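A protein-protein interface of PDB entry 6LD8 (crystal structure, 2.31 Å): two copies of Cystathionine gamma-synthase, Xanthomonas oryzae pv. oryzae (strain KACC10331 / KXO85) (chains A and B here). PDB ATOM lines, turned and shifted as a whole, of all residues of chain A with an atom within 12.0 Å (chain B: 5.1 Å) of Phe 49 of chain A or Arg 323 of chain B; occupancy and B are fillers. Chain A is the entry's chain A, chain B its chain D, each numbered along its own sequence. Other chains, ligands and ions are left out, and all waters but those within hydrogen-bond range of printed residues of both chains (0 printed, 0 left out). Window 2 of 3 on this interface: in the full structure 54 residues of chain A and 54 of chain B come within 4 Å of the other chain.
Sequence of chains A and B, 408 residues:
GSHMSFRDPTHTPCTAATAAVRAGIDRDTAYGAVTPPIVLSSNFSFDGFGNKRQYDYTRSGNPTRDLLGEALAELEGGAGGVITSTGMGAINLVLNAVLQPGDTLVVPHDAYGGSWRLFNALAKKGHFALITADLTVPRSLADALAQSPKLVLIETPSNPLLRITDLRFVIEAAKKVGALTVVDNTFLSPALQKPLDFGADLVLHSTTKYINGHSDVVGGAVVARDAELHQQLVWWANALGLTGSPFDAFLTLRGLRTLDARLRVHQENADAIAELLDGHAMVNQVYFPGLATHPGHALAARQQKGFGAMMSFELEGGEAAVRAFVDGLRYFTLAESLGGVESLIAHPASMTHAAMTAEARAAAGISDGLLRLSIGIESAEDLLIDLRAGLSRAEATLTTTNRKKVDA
Among the printed residues, pairs that only touch across the chains: Ser 45 of chain A with Leu 334 of chain B (3.3 Å), Phe 49 of chain A with His 347 of chain B (3.7 Å), Phe 49 of chain A with Leu 334 of chain B (3.7 Å), Gly 48 of chain A with Leu 334 of chain B (3.7 Å), Phe 49 of chain A with Arg 323 of chain B (3.8 Å) and Phe 49 of chain A with Val 322 of chain B (3.8 Å).
The guanidinium group of Arg 53 of chain A lies within hydrogen-bond range of the backbone carbonyl oxygen of Ser 45 of chain A, at 2.8 Å.
NH2 of Arg 323 of chain B is in salt-bridge range of OE2 of Glu 319 of chain B, 2.6 Å away.
Hydrophobic or aromatic side chains of chain A that line the printed part of chain B: Phe 46 and Phe 49.
Among the printed residues, 7 pairs touch across the chains.
Among the printed residues, no Asp or Glu carboxylate lies within 4 Å of a Lys or Arg side-chain nitrogen of the other chain.
The backbone NH (N) of Phe 46 of chain A sits at hydrogen-bond distance from the backbone carbonyl oxygen (O) of Leu 334 of chain B (2.9 Å).
Phe 49 of chain A touches just these residues of chain B: Val 322, Arg 323, Leu 334 and His 347.
Of chain A, only Phe 49 (3.8 Å) comes within 4 Å of Arg 323 of chain B.
No residue of chain A comes within 4 Å of Glu 319 of chain B.
No residue of chain A comes within 4 Å of Ala 320 of chain B.
No residue of chain A comes within 4 Å of Ala 324 of chain B.
No residue of chain A comes within 4 Å of Asp 327 of chain B.
Of the printed residues of chain A, His 347 of chain B touches Phe 49 (3.7 Å).
Of the printed residues of chain A, Leu 334 of chain B touches Ser 45 (3.3 Å), Phe 46 (2.9 Å), Gly 48 (3.7 Å) and Phe 49 (3.7 Å).
Printed residues of chain B within 4 Å of Ser 45 of chain A: Leu 334.
Of the printed residues of chain B, Phe 46 of chain A touches Leu 334.
Printed residues of chain B within 4 Å of Gly 48 of chain A: Leu 334 (3.7 Å).
Asp 47 of chain A touches none of the printed residues of chain B.
Lys 52 of chain A touches none of the printed residues of chain B.
The nearest residue of chain B that does not touch Phe 49 of chain A is Val 326 of chain B (4.4 Å).
The nearest residue of chain A that does not touch Arg 323 of chain B is Gly 50 of chain A (5.7 Å).
No position is printed for both chains.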
ATOM      1  N   PHE A  44      -3.700 -35.747 -18.722  1.00  0.00           N
ATOM      2  CA  PHE A  44      -3.418 -36.671 -19.848  1.00  0.00           C
ATOM      3  C   PHE A  44      -3.312 -35.788 -21.083  1.00  0.00           C
ATOM      4  O   PHE A  44      -4.095 -34.874 -21.185  1.00  0.00           O
ATOM      5  CB  PHE A  44      -4.562 -37.687 -19.987  1.00  0.00           C
ATOM      6  CG  PHE A  44      -4.745 -38.527 -18.757  1.00  0.00           C
ATOM      7  CD1 PHE A  44      -5.389 -38.018 -17.662  1.00  0.00           C
ATOM      8  CD2 PHE A  44      -4.186 -39.799 -18.669  1.00  0.00           C
ATOM      9  CE1 PHE A  44      -5.509 -38.764 -16.496  1.00  0.00           C
ATOM     10  CE2 PHE A  44      -4.309 -40.546 -17.519  1.00  0.00           C
ATOM     11  CZ  PHE A  44      -4.953 -40.021 -16.429  1.00  0.00           C
ATOM     12  N   SER A  45      -2.383 -36.046 -21.982  1.00  0.00           N
ATOM     13  CA  SER A  45      -2.234 -35.242 -23.210  1.00  0.00           C
ATOM     14  C   SER A  45      -3.440 -35.482 -24.127  1.00  0.00           C
ATOM     15  O   SER A  45      -4.023 -36.579 -24.077  1.00  0.00           O
ATOM     16  CB  SER A  45      -0.938 -35.573 -23.887  1.00  0.00           C
ATOM     17  OG  SER A  45      -0.918 -36.919 -24.250  1.00  0.00           O
ATOM     18  N   PHE A  46      -3.808 -34.468 -24.908  1.00  0.00           N
ATOM     19  CA  PHE A  46      -4.698 -34.598 -26.092  1.00  0.00           C
ATOM     20  C   PHE A  46      -3.909 -35.255 -27.224  1.00  0.00           C
ATOM     21  O   PHE A  46      -2.669 -35.204 -27.183  1.00  0.00           O
ATOM     22  CB  PHE A  46      -5.319 -33.251 -26.467  1.00  0.00           C
ATOM     23  CG  PHE A  46      -6.487 -32.876 -25.611  1.00  0.00           C
ATOM     24  CD1 PHE A  46      -6.468 -33.108 -24.257  1.00  0.00           C
ATOM     25  CD2 PHE A  46      -7.625 -32.316 -26.168  1.00  0.00           C
ATOM     26  CE1 PHE A  46      -7.554 -32.775 -23.467  1.00  0.00           C
ATOM     27  CE2 PHE A  46      -8.721 -31.984 -25.383  1.00  0.00           C
ATOM     28  CZ  PHE A  46      -8.681 -32.216 -24.031  1.00  0.00           C
ATOM     29  N   ASP A  47      -4.590 -35.948 -28.146  1.00  0.00           N
ATOM     30  CA  ASP A  47      -3.925 -36.621 -29.302  1.00  0.00           C
ATOM     31  C   ASP A  47      -3.837 -35.625 -30.476  1.00  0.00           C
ATOM     32  O   ASP A  47      -4.389 -35.916 -31.548  1.00  0.00           O
ATOM     33  CB  ASP A  47      -4.628 -37.937 -29.661  1.00  0.00           C
ATOM     34  CG  ASP A  47      -3.877 -38.807 -30.674  1.00  0.00           C
ATOM     35  OD1 ASP A  47      -2.647 -38.615 -30.845  1.00  0.00           O
ATOM     36  OD2 ASP A  47      -4.529 -39.687 -31.279  1.00  0.00           O
ATOM     37  N   GLY A  48      -3.129 -34.511 -30.283  1.00  0.00           N
ATOM     38  CA  GLY A  48      -3.191 -33.331 -31.163  1.00  0.00           C
ATOM     39  C   GLY A  48      -4.461 -32.504 -30.937  1.00  0.00           C
ATOM     40  O   GLY A  48      -5.406 -32.950 -30.217  1.00  0.00           O
ATOM     41  N   PHE A  49      -4.480 -31.309 -31.530  1.00  0.00           N
ATOM     42  CA  PHE A  49      -5.549 -30.292 -31.362  1.00  0.00           C
ATOM     43  C   PHE A  49      -6.944 -30.919 -31.576  1.00  0.00           C
ATOM     44  O   PHE A  49      -7.175 -31.574 -32.624  1.00  0.00           O
ATOM     45  CB  PHE A  49      -5.305 -29.100 -32.299  1.00  0.00           C
ATOM     46  CG  PHE A  49      -6.228 -27.948 -32.000  1.00  0.00           C
ATOM     47  CD1 PHE A  49      -6.094 -27.230 -30.817  1.00  0.00           C
ATOM     48  CD2 PHE A  49      -7.294 -27.650 -32.840  1.00  0.00           C
ATOM     49  CE1 PHE A  49      -6.962 -26.190 -30.523  1.00  0.00           C
ATOM     50  CE2 PHE A  49      -8.156 -26.604 -32.546  1.00  0.00           C
ATOM     51  CZ  PHE A  49      -7.984 -25.870 -31.393  1.00  0.00           C
ATOM     52  N   GLY A  50      -7.853 -30.677 -30.624  1.00  0.00           N
ATOM     53  CA  GLY A  50      -9.282 -31.049 -30.679  1.00  0.00           C
ATOM     54  C   GLY A  50      -9.558 -32.513 -30.304  1.00  0.00           C
ATOM     55  O   GLY A  50     -10.751 -32.852 -30.233  1.00  0.00           O
ATOM     56  N   ASN A  51      -8.533 -33.349 -30.036  1.00  0.00           N
ATOM     57  CA  ASN A  51      -8.685 -34.825 -29.864  1.00  0.00           C
ATOM     58  C   ASN A  51      -8.409 -35.232 -28.404  1.00  0.00           C
ATOM     59  O   ASN A  51      -7.272 -35.646 -28.110  1.00  0.00           O
ATOM     60  CB  ASN A  51      -7.811 -35.612 -30.860  1.00  0.00           C
ATOM     61  CG  ASN A  51      -7.961 -35.121 -32.291  1.00  0.00           C
ATOM     62  OD1 ASN A  51      -6.989 -35.071 -33.045  1.00  0.00           O
ATOM     63  ND2 ASN A  51      -9.165 -34.706 -32.663  1.00  0.00           N
ATOM     64  N   LYS A  52      -9.412 -35.119 -27.526  1.00  0.00           N
ATOM     65  CA  LYS A  52      -9.445 -35.719 -26.161  1.00  0.00           C
ATOM     66  C   LYS A  52      -9.148 -37.217 -26.308  1.00  0.00           C
ATOM     67  O   LYS A  52      -9.574 -37.802 -27.257  1.00  0.00           O
ATOM     68  CB  LYS A  52     -10.823 -35.525 -25.511  1.00  0.00           C
ATOM     69  CG  LYS A  52     -10.843 -35.511 -23.989  1.00  0.00           C
ATOM     70  CD  LYS A  52     -12.224 -35.206 -23.361  1.00  0.00           C
ATOM     71  CE  LYS A  52     -13.210 -36.366 -23.351  1.00  0.00           C
ATOM     72  NZ  LYS A  52     -12.615 -37.642 -22.878  1.00  0.00           N
ATOM     73  N   ARG A  53      -8.369 -37.803 -25.420  1.00  0.00           N
ATOM     74  CA  ARG A  53      -8.202 -39.269 -25.334  1.00  0.00           C
ATOM     75  C   ARG A  53      -9.347 -39.808 -24.454  1.00  0.00           C
ATOM     76  O   ARG A  53     -10.204 -38.992 -23.989  1.00  0.00           O
ATOM     77  CB  ARG A  53      -6.809 -39.565 -24.759  1.00  0.00           C
ATOM     78  CG  ARG A  53      -5.633 -39.265 -25.683  1.00  0.00           C
ATOM     79  CD  ARG A  53      -4.372 -39.581 -24.912  1.00  0.00           C
ATOM     80  NE  ARG A  53      -3.208 -38.859 -25.395  1.00  0.00           N
ATOM     81  CZ  ARG A  53      -2.474 -39.234 -26.423  1.00  0.00           C
ATOM     82  NH1 ARG A  53      -2.791 -40.310 -27.126  1.00  0.00           N
ATOM     83  NH2 ARG A  53      -1.438 -38.507 -26.792  1.00  0.00           N
ATOM     84  N   GLU B 319      -8.364 -20.116 -36.997  1.00  0.00           N
ATOM     85  CA  GLU B 319      -8.266 -21.505 -36.481  1.00  0.00           C
ATOM     86  C   GLU B 319      -7.066 -22.214 -37.124  1.00  0.00           C
ATOM     87  O   GLU B 319      -6.415 -23.040 -36.432  1.00  0.00           O
ATOM     88  CB  GLU B 319      -9.566 -22.289 -36.692  1.00  0.00           C
ATOM     89  CG  GLU B 319      -9.682 -23.454 -35.723  1.00  0.00           C
ATOM     90  CD  GLU B 319     -10.834 -24.411 -35.959  1.00  0.00           C
ATOM     91  OE1 GLU B 319     -11.783 -24.406 -35.146  1.00  0.00           O
ATOM     92  OE2 GLU B 319     -10.750 -25.187 -36.929  1.00  0.00           O
ATOM     93  N   ALA B 320      -6.752 -21.908 -38.380  1.00  0.00           N
ATOM     94  CA  ALA B 320      -5.679 -22.626 -39.101  1.00  0.00           C
ATOM     95  C   ALA B 320      -4.338 -22.308 -38.418  1.00  0.00           C
ATOM     96  O   ALA B 320      -3.496 -23.183 -38.397  1.00  0.00           O
ATOM     97  CB  ALA B 320      -5.689 -22.283 -40.573  1.00  0.00           C
ATOM     98  N   ALA B 321      -4.175 -21.088 -37.906  1.00  0.00           N
ATOM     99  CA  ALA B 321      -2.950 -20.589 -37.240  1.00  0.00           C
ATOM    100  C   ALA B 321      -2.811 -21.318 -35.896  1.00  0.00           C
ATOM    101  O   ALA B 321      -1.731 -21.858 -35.604  1.00  0.00           O
ATOM    102  CB  ALA B 321      -3.027 -19.084 -37.058  1.00  0.00           C
ATOM    103  N   VAL B 322      -3.896 -21.365 -35.130  1.00  0.00           N
ATOM    104  CA  VAL B 322      -3.933 -22.094 -33.838  1.00  0.00           C
ATOM    105  C   VAL B 322      -3.477 -23.527 -34.065  1.00  0.00           C
ATOM    106  O   VAL B 322      -2.625 -23.950 -33.320  1.00  0.00           O
ATOM    107  CB  VAL B 322      -5.327 -22.044 -33.211  1.00  0.00           C
ATOM    108  CG1 VAL B 322      -5.479 -23.114 -32.140  1.00  0.00           C
ATOM    109  CG2 VAL B 322      -5.625 -20.650 -32.667  1.00  0.00           C
ATOM    110  N   ARG B 323      -4.012 -24.211 -35.073  1.00  0.00           N
ATOM    111  CA  ARG B 323      -3.771 -25.657 -35.314  1.00  0.00           C
ATOM    112  C   ARG B 323      -2.290 -25.818 -35.673  1.00  0.00           C
ATOM    113  O   ARG B 323      -1.655 -26.752 -35.143  1.00  0.00           O
ATOM    114  CB  ARG B 323      -4.753 -26.245 -36.350  1.00  0.00           C
ATOM    115  CG  ARG B 323      -4.666 -27.760 -36.584  1.00  0.00           C
ATOM    116  CD  ARG B 323      -5.825 -28.364 -37.402  1.00  0.00           C
ATOM    117  NE  ARG B 323      -7.096 -27.615 -37.253  1.00  0.00           N
ATOM    118  CZ  ARG B 323      -8.214 -28.038 -36.627  1.00  0.00           C
ATOM    119  NH1 ARG B 323      -8.294 -29.242 -36.091  1.00  0.00           N
ATOM    120  NH2 ARG B 323      -9.267 -27.242 -36.535  1.00  0.00           N
ATOM    121  N   ALA B 324      -1.739 -24.939 -36.507  1.00  0.00           N
ATOM    122  CA  ALA B 324      -0.340 -25.066 -36.966  1.00  0.00           C
ATOM    123  C   ALA B 324       0.628 -24.752 -35.807  1.00  0.00           C
ATOM    124  O   ALA B 324       1.623 -25.461 -35.662  1.00  0.00           O
ATOM    125  CB  ALA B 324      -0.110 -24.154 -38.140  1.00  0.00           C
ATOM    126  N   PHE B 325       0.373 -23.700 -35.032  1.00  0.00           N
ATOM    127  CA  PHE B 325       1.145 -23.365 -33.810  1.00  0.00           C
ATOM    128  C   PHE B 325       1.206 -24.595 -32.894  1.00  0.00           C
ATOM    129  O   PHE B 325       2.304 -24.986 -32.522  1.00  0.00           O
ATOM    130  CB  PHE B 325       0.513 -22.193 -33.066  1.00  0.00           C
ATOM    131  CG  PHE B 325       1.306 -21.728 -31.877  1.00  0.00           C
ATOM    132  CD1 PHE B 325       1.117 -22.292 -30.620  1.00  0.00           C
ATOM    133  CD2 PHE B 325       2.227 -20.707 -32.004  1.00  0.00           C
ATOM    134  CE1 PHE B 325       1.839 -21.850 -29.518  1.00  0.00           C
ATOM    135  CE2 PHE B 325       2.981 -20.302 -30.917  1.00  0.00           C
ATOM    136  CZ  PHE B 325       2.788 -20.866 -29.680  1.00  0.00           C
ATOM    137  N   VAL B 326       0.060 -25.189 -32.548  1.00  0.00           N
ATOM    138  CA  VAL B 326      -0.050 -26.242 -31.491  1.00  0.00           C
ATOM    139  C   VAL B 326       0.600 -27.541 -31.993  1.00  0.00           C
ATOM    140  O   VAL B 326       1.377 -28.130 -31.228  1.00  0.00           O
ATOM    141  CB  VAL B 326      -1.508 -26.442 -31.041  1.00  0.00           C
ATOM    142  CG1 VAL B 326      -1.696 -27.697 -30.218  1.00  0.00           C
ATOM    143  CG2 VAL B 326      -2.023 -25.249 -30.258  1.00  0.00           C
ATOM    144  N   ASP B 327       0.327 -27.968 -33.226  1.00  0.00           N
ATOM    145  CA  ASP B 327       0.956 -29.176 -33.837  1.00  0.00           C
ATOM    146  C   ASP B 327       2.444 -28.858 -33.985  1.00  0.00           C
ATOM    147  O   ASP B 327       2.793 -27.984 -34.778  1.00  0.00           O
ATOM    148  CB  ASP B 327       0.321 -29.583 -35.189  1.00  0.00           C
ATOM    149  CG  ASP B 327       1.062 -30.654 -36.017  1.00  0.00           C
ATOM    150  OD1 ASP B 327       1.604 -31.611 -35.414  1.00  0.00           O
ATOM    151  OD2 ASP B 327       1.082 -30.550 -37.283  1.00  0.00           O
ATOM    152  N   LEU B 334       0.023 -30.378 -24.821  1.00  0.00           N
ATOM    153  CA  LEU B 334      -1.410 -29.969 -24.912  1.00  0.00           C
ATOM    154  C   LEU B 334      -2.214 -30.818 -23.932  1.00  0.00           C
ATOM    155  O   LEU B 334      -2.347 -32.049 -24.130  1.00  0.00           O
ATOM    156  CB  LEU B 334      -1.849 -30.187 -26.349  1.00  0.00           C
ATOM    157  CG  LEU B 334      -3.305 -29.886 -26.663  1.00  0.00           C
ATOM    158  CD1 LEU B 334      -3.638 -28.451 -26.333  1.00  0.00           C
ATOM    159  CD2 LEU B 334      -3.559 -30.197 -28.130  1.00  0.00           C
ATOM    160  N   HIS B 347      -6.278 -24.951 -24.905  1.00  0.00           N
ATOM    161  CA  HIS B 347      -7.315 -24.187 -25.660  1.00  0.00           C
ATOM    162  C   HIS B 347      -8.620 -24.233 -24.852  1.00  0.00           C
ATOM    163  O   HIS B 347      -9.366 -25.223 -24.934  1.00  0.00           O
ATOM    164  CB  HIS B 347      -7.432 -24.782 -27.058  1.00  0.00           C
ATOM    165  CG  HIS B 347      -8.571 -24.267 -27.863  1.00  0.00           C
ATOM    166  ND1 HIS B 347      -9.804 -24.901 -27.865  1.00  0.00           N
ATOM    167  CD2 HIS B 347      -8.636 -23.254 -28.759  1.00  0.00           C
ATOM    168  CE1 HIS B 347     -10.614 -24.249 -28.658  1.00  0.00           C
ATOM    169  NE2 HIS B 347      -9.915 -23.229 -29.219  1.00  0.00           N
